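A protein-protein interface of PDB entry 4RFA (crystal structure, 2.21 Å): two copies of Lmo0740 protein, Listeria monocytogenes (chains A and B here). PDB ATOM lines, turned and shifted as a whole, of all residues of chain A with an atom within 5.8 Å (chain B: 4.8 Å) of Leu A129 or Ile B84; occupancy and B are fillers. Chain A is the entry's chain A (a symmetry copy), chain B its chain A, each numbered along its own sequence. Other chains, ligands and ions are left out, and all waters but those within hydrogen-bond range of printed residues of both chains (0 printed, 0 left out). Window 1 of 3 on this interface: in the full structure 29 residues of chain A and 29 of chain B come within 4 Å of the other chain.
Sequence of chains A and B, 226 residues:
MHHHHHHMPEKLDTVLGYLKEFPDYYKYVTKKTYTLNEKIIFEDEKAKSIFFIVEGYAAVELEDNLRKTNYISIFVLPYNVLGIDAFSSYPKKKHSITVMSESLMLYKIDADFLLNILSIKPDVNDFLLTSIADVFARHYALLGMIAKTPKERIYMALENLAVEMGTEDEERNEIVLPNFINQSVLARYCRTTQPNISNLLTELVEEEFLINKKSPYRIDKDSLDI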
ATOM      1  N   ASN A 125     -10.998   5.471  -7.637  1.00  0.00           N
ATOM      2  CA  ASN A 125     -10.585   5.068  -8.968  1.00  0.00           C
ATOM      3  C   ASN A 125     -11.230   3.738  -9.331  1.00  0.00           C
ATOM      4  O   ASN A 125     -11.363   3.409 -10.511  1.00  0.00           O
ATOM      5  CB  ASN A 125      -9.055   4.961  -9.018  1.00  0.00           C
ATOM      6  CG  ASN A 125      -8.500   4.966 -10.428  1.00  0.00           C
ATOM      7  OD1 ASN A 125      -9.199   5.290 -11.393  1.00  0.00           O
ATOM      8  ND2 ASN A 125      -7.221   4.609 -10.552  1.00  0.00           N
ATOM      9  N   ASP A 126     -11.624   2.983  -8.300  1.00  0.00           N
ATOM     10  CA  ASP A 126     -12.318   1.732  -8.478  1.00  0.00           C
ATOM     11  C   ASP A 126     -13.360   1.925  -9.508  1.00  0.00           C
ATOM     12  O   ASP A 126     -13.564   1.029 -10.331  1.00  0.00           O
ATOM     13  CB  ASP A 126     -12.979   1.231  -7.199  1.00  0.00           C
ATOM     14  CG  ASP A 126     -11.964   0.763  -6.209  1.00  0.00           C
ATOM     15  OD1 ASP A 126     -10.800   0.562  -6.616  1.00  0.00           O
ATOM     16  OD2 ASP A 126     -12.326   0.555  -5.031  1.00  0.00           O
ATOM     17  N   PHE A 127     -14.004   3.093  -9.448  1.00  0.00           N
ATOM     18  CA  PHE A 127     -15.033   3.419 -10.396  1.00  0.00           C
ATOM     19  C   PHE A 127     -14.540   3.390 -11.845  1.00  0.00           C
ATOM     20  O   PHE A 127     -15.218   2.888 -12.697  1.00  0.00           O
ATOM     21  CB  PHE A 127     -15.655   4.785 -10.139  1.00  0.00           C
ATOM     22  CG  PHE A 127     -16.744   5.073 -11.088  1.00  0.00           C
ATOM     23  CD1 PHE A 127     -17.922   4.372 -11.001  1.00  0.00           C
ATOM     24  CD2 PHE A 127     -16.555   5.940 -12.144  1.00  0.00           C
ATOM     25  CE1 PHE A 127     -18.938   4.576 -11.917  1.00  0.00           C
ATOM     26  CE2 PHE A 127     -17.559   6.141 -13.071  1.00  0.00           C
ATOM     27  CZ  PHE A 127     -18.748   5.447 -12.965  1.00  0.00           C
ATOM     28  N   LEU A 128     -13.394   3.980 -12.114  1.00  0.00           N
ATOM     29  CA  LEU A 128     -12.905   4.036 -13.473  1.00  0.00           C
ATOM     30  C   LEU A 128     -12.429   2.643 -13.987  1.00  0.00           C
ATOM     31  O   LEU A 128     -12.790   2.220 -15.086  1.00  0.00           O
ATOM     32  CB  LEU A 128     -11.803   5.082 -13.582  1.00  0.00           C
ATOM     33  CG  LEU A 128     -11.108   5.212 -14.942  1.00  0.00           C
ATOM     34  CD1 LEU A 128     -12.112   5.416 -16.059  1.00  0.00           C
ATOM     35  CD2 LEU A 128     -10.116   6.357 -14.901  1.00  0.00           C
ATOM     36  N   LEU A 129     -11.650   1.971 -13.157  1.00  0.00           N
ATOM     37  CA  LEU A 129     -11.161   0.622 -13.387  1.00  0.00           C
ATOM     38  C   LEU A 129     -12.280  -0.359 -13.605  1.00  0.00           C
ATOM     39  O   LEU A 129     -12.212  -1.173 -14.508  1.00  0.00           O
ATOM     40  CB  LEU A 129     -10.383   0.138 -12.167  1.00  0.00           C
ATOM     41  CG  LEU A 129      -8.996   0.725 -11.995  1.00  0.00           C
ATOM     42  CD1 LEU A 129      -8.345   0.033 -10.804  1.00  0.00           C
ATOM     43  CD2 LEU A 129      -8.157   0.547 -13.257  1.00  0.00           C
ATOM     44  N   THR A 130     -13.307  -0.269 -12.776  1.00  0.00           N
ATOM     45  CA  THR A 130     -14.486  -1.123 -12.895  1.00  0.00           C
ATOM     46  C   THR A 130     -15.236  -0.883 -14.162  1.00  0.00           C
ATOM     47  O   THR A 130     -15.654  -1.832 -14.788  1.00  0.00           O
ATOM     48  CB  THR A 130     -15.422  -0.963 -11.684  1.00  0.00           C
ATOM     49  OG1 THR A 130     -14.747  -1.474 -10.532  1.00  0.00           O
ATOM     50  CG2 THR A 130     -16.724  -1.729 -11.883  1.00  0.00           C
ATOM     51  N   SER A 131     -15.398   0.374 -14.560  1.00  0.00           N
ATOM     52  CA  SER A 131     -16.045   0.693 -15.823  1.00  0.00           C
ATOM     53  C   SER A 131     -15.310   0.100 -17.027  1.00  0.00           C
ATOM     54  O   SER A 131     -15.940  -0.430 -17.930  1.00  0.00           O
ATOM     55  CB  SER A 131     -16.121   2.199 -16.022  1.00  0.00           C
ATOM     56  OG  SER A 131     -16.432   2.816 -14.805  1.00  0.00           O
ATOM     57  N   ILE A 132     -13.991   0.230 -17.024  1.00  0.00           N
ATOM     58  CA  ILE A 132     -13.113  -0.328 -18.047  1.00  0.00           C
ATOM     59  C   ILE A 132     -13.224  -1.839 -18.053  1.00  0.00           C
ATOM     60  O   ILE A 132     -13.520  -2.422 -19.091  1.00  0.00           O
ATOM     61  CB  ILE A 132     -11.632   0.072 -17.772  1.00  0.00           C
ATOM     62  CG1 ILE A 132     -11.415   1.592 -17.852  1.00  0.00           C
ATOM     63  CG2 ILE A 132     -10.668  -0.592 -18.732  1.00  0.00           C
ATOM     64  CD1 ILE A 132     -12.397   2.330 -18.715  1.00  0.00           C
ATOM     65  N   ALA A 133     -13.027  -2.443 -16.880  1.00  0.00           N
ATOM     66  CA  ALA A 133     -13.159  -3.904 -16.671  1.00  0.00           C
ATOM     67  C   ALA A 133     -14.423  -4.429 -17.280  1.00  0.00           C
ATOM     68  O   ALA A 133     -14.405  -5.425 -17.987  1.00  0.00           O
ATOM     69  CB  ALA A 133     -13.129  -4.225 -15.186  1.00  0.00           C
ATOM     70  N   ASP A 134     -15.541  -3.728 -17.087  1.00  0.00           N
ATOM     71  CA  ASP A 134     -16.798  -4.212 -17.683  1.00  0.00           C
ATOM     72  C   ASP A 134     -16.805  -4.102 -19.204  1.00  0.00           C
ATOM     73  O   ASP A 134     -17.422  -4.912 -19.864  1.00  0.00           O
ATOM     74  CB  ASP A 134     -18.004  -3.473 -17.101  1.00  0.00           C
ATOM     75  CG  ASP A 134     -18.248  -3.835 -15.651  1.00  0.00           C
ATOM     76  OD1 ASP A 134     -17.765  -4.893 -15.211  1.00  0.00           O
ATOM     77  OD2 ASP A 134     -18.934  -3.074 -14.951  1.00  0.00           O
ATOM     78  N   PHE A 136     -14.128  -4.421 -21.173  1.00  0.00           N
ATOM     79  CA  PHE A 136     -13.321  -5.603 -21.484  1.00  0.00           C
ATOM     80  C   PHE A 136     -14.092  -6.895 -21.472  1.00  0.00           C
ATOM     81  O   PHE A 136     -13.999  -7.687 -22.418  1.00  0.00           O
ATOM     82  CB  PHE A 136     -12.187  -5.754 -20.511  1.00  0.00           C
ATOM     83  CG  PHE A 136     -11.111  -4.761 -20.713  1.00  0.00           C
ATOM     84  CD1 PHE A 136     -10.941  -4.135 -21.924  1.00  0.00           C
ATOM     85  CD2 PHE A 136     -10.259  -4.457 -19.690  1.00  0.00           C
ATOM     86  CE1 PHE A 136      -9.920  -3.214 -22.111  1.00  0.00           C
ATOM     87  CE2 PHE A 136      -9.238  -3.551 -19.878  1.00  0.00           C
ATOM     88  CZ  PHE A 136      -9.066  -2.925 -21.088  1.00  0.00           C
ATOM     89  N   ILE B  50      -2.577  -4.813 -10.255  1.00  0.00           N
ATOM     90  CA  ILE B  50      -2.446  -4.675 -11.680  1.00  0.00           C
ATOM     91  C   ILE B  50      -1.115  -5.350 -12.059  1.00  0.00           C
ATOM     92  O   ILE B  50      -0.178  -5.312 -11.268  1.00  0.00           O
ATOM     93  CB  ILE B  50      -2.450  -3.179 -12.017  1.00  0.00           C
ATOM     94  CG1 ILE B  50      -3.759  -2.548 -11.559  1.00  0.00           C
ATOM     95  CG2 ILE B  50      -2.294  -2.941 -13.488  1.00  0.00           C
ATOM     96  CD1 ILE B  50      -4.989  -3.279 -12.064  1.00  0.00           C
ATOM     97  N   VAL B  81      -1.035  -4.011 -19.649  1.00  0.00           N
ATOM     98  CA  VAL B  81      -1.544  -4.107 -18.279  1.00  0.00           C
ATOM     99  C   VAL B  81      -2.436  -5.340 -18.217  1.00  0.00           C
ATOM    100  O   VAL B  81      -3.074  -5.614 -19.196  1.00  0.00           O
ATOM    101  CB  VAL B  81      -2.378  -2.873 -17.882  1.00  0.00           C
ATOM    102  CG1 VAL B  81      -2.499  -2.788 -16.388  1.00  0.00           C
ATOM    103  CG2 VAL B  81      -1.718  -1.613 -18.369  1.00  0.00           C
ATOM    104  N   LEU B  82      -2.453  -6.082 -17.104  1.00  0.00           N
ATOM    105  CA  LEU B  82      -3.252  -7.313 -16.971  1.00  0.00           C
ATOM    106  C   LEU B  82      -3.950  -7.284 -15.635  1.00  0.00           C
ATOM    107  O   LEU B  82      -3.568  -6.549 -14.678  1.00  0.00           O
ATOM    108  CB  LEU B  82      -2.419  -8.601 -16.998  1.00  0.00           C
ATOM    109  CG  LEU B  82      -2.105  -9.444 -18.216  1.00  0.00           C
ATOM    110  CD1 LEU B  82      -1.211 -10.609 -17.883  1.00  0.00           C
ATOM    111  CD2 LEU B  82      -3.335  -9.997 -18.905  1.00  0.00           C
ATOM    112  N   GLY B  83      -5.009  -8.080 -15.582  1.00  0.00           N
ATOM    113  CA  GLY B  83      -5.797  -8.211 -14.380  1.00  0.00           C
ATOM    114  C   GLY B  83      -6.809  -7.104 -14.174  1.00  0.00           C
ATOM    115  O   GLY B  83      -7.312  -6.938 -13.055  1.00  0.00           O
ATOM    116  N   ILE B  84      -7.107  -6.320 -15.207  1.00  0.00           N
ATOM    117  CA  ILE B  84      -8.142  -5.257 -15.048  1.00  0.00           C
ATOM    118  C   ILE B  84      -9.518  -5.915 -14.962  1.00  0.00           C
ATOM    119  O   ILE B  84     -10.410  -5.440 -14.266  1.00  0.00           O
ATOM    120  CB  ILE B  84      -8.177  -4.220 -16.178  1.00  0.00           C
ATOM    121  CG1 ILE B  84      -6.790  -3.619 -16.432  1.00  0.00           C
ATOM    122  CG2 ILE B  84      -9.206  -3.129 -15.854  1.00  0.00           C
ATOM    123  CD1 ILE B  84      -6.384  -2.480 -15.565  1.00  0.00           C
ATOM    124  N   ASP B  85      -9.651  -7.030 -15.655  1.00  0.00           N
ATOM    125  CA  ASP B  85     -10.837  -7.886 -15.613  1.00  0.00           C
ATOM    126  C   ASP B  85     -11.307  -8.224 -14.231  1.00  0.00           C
ATOM    127  O   ASP B  85     -12.508  -8.388 -13.994  1.00  0.00           O
ATOM    128  CB  ASP B  85     -10.562  -9.187 -16.373  1.00  0.00           C
ATOM    129  CG  ASP B  85     -10.409  -8.971 -17.856  1.00  0.00           C
ATOM    130  OD1 ASP B  85     -10.881  -7.933 -18.380  1.00  0.00           O
ATOM    131  OD2 ASP B  85      -9.829  -9.851 -18.520  1.00  0.00           O
ATOM    132  N   ALA B  86     -10.386  -8.297 -13.294  1.00  0.00           N
ATOM    133  CA  ALA B  86     -10.733  -8.654 -11.935  1.00  0.00           C
ATOM    134  C   ALA B  86     -11.530  -7.606 -11.198  1.00  0.00           C
ATOM    135  O   ALA B  86     -12.103  -7.874 -10.131  1.00  0.00           O
ATOM    136  CB  ALA B  86      -9.459  -8.945 -11.173  1.00  0.00           C
ATOM    137  N   PHE B  87     -11.532  -6.386 -11.726  1.00  0.00           N
ATOM    138  CA  PHE B  87     -12.317  -5.323 -11.151  1.00  0.00           C
ATOM    139  C   PHE B  87     -13.733  -5.314 -11.676  1.00  0.00           C
ATOM    140  O   PHE B  87     -14.559  -4.578 -11.196  1.00  0.00           O
ATOM    141  CB  PHE B  87     -11.638  -3.984 -11.432  1.00  0.00           C
ATOM    142  CG  PHE B  87     -10.371  -3.814 -10.664  1.00  0.00           C
ATOM    143  CD1 PHE B  87      -9.206  -4.423 -11.088  1.00  0.00           C
ATOM    144  CD2 PHE B  87     -10.373  -3.104  -9.470  1.00  0.00           C
ATOM    145  CE1 PHE B  87      -8.042  -4.306 -10.357  1.00  0.00           C
ATOM    146  CE2 PHE B  87      -9.209  -2.973  -8.734  1.00  0.00           C
ATOM    147  CZ  PHE B  87      -8.044  -3.570  -9.177  1.00  0.00           C
ATOM    148  N   SER B  88     -14.019  -6.141 -12.652  1.00  0.00           N
ATOM    149  CA  SER B  88     -15.302  -6.061 -13.337  1.00  0.00           C
ATOM    150  C   SER B  88     -16.400  -6.630 -12.480  1.00  0.00           C
ATOM    151  O   SER B  88     -16.214  -7.665 -11.868  1.00  0.00           O
ATOM    152  CB  SER B  88     -15.301  -6.873 -14.614  1.00  0.00           C
ATOM    153  OG  SER B  88     -15.516  -8.233 -14.280  1.00  0.00           O
ATOM    154  N   ILE B 132      -4.351   0.869 -21.729  1.00  0.00           N
ATOM    155  CA  ILE B 132      -5.727   0.401 -21.864  1.00  0.00           C
ATOM    156  C   ILE B 132      -6.222   0.660 -23.272  1.00  0.00           C
ATOM    157  O   ILE B 132      -6.660  -0.269 -23.942  1.00  0.00           O
ATOM    158  CB  ILE B 132      -6.656   1.140 -20.854  1.00  0.00           C
ATOM    159  CG1 ILE B 132      -6.280   0.843 -19.393  1.00  0.00           C
ATOM    160  CG2 ILE B 132      -8.115   0.783 -21.046  1.00  0.00           C
ATOM    161  CD1 ILE B 132      -5.573  -0.464 -19.172  1.00  0.00           C
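Of the printed residues of chain B, Ala A133 touches Ile B84 (3.1 Å), Phe B87 (3.7 Å) and Ser B88 (3.3 Å).
Of chain A, only Leu A129, Ala A133 and Phe A136 come within 4 Å of Ile B84.
Printed residues of chain A within 4 Å of Asp B85: Phe A136 (3.3 Å).
Of the printed residues of chain A, Ser B88 touches Ala A133 and Asp A134.
Printed residues of chain A within 4 Å of Ile B132: Ile A132 and Phe A136.
The nearest printed residue of chain B that does not touch Leu A129 is Ile B50 (4.9 Å).
Among the printed residues, merely in contact across the chains: Ala A133 with Ile B84 (3.1 Å), Asp A134 with Ser B88 (3.2 Å), Ala A133 with Ser B88 (3.3 Å), Phe A136 with Asp B85 (3.3 Å), Ile A132 with Ile B132 (3.7 Å), Ala A133 with Phe B87 (3.7 Å), Leu A129 with Phe B87 (3.8 Å), Phe A136 with Ile B132 (3.8 Å), Leu A129 with Ile B84 (3.8 Å) and Phe A136 with Ile B84 (3.9 Å).
The side-chain hydroxyl (OG) of Ser B88 sits at hydrogen-bond distance from the backbone carbonyl oxygen (O) of Asp B85, at 3.0 Å.
O of Asp A126 sits at hydrogen-bond distance from OG1 of Thr A130.
Of the 10 printed residues of chain B, 5 touch a printed residue of chain A.
Printed residues of chain B that touch a printed residue of chain A: Ile B84, Asp B85, Phe B87, Ser B88 and Ile B132.
Hydrophobic or aromatic side chains of chain A that line the printed part of chain B: Leu A129, Ile A132, Ala A133 and Phe A136.
Among the printed residues, 11 pairs touch across the chains.
Among the printed residues, no Asp or Glu carboxylate lies within 4 Å of a Lys or Arg side-chain nitrogen of the other chain.
Ile B132 touches its own counterpart, Ile A132.
Position printed for both chains: 132.
The side-chain hydroxyl of Thr A130 is in hydrogen-bond range of the backbone carbonyl oxygen of Phe B87 (3.2 Å).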
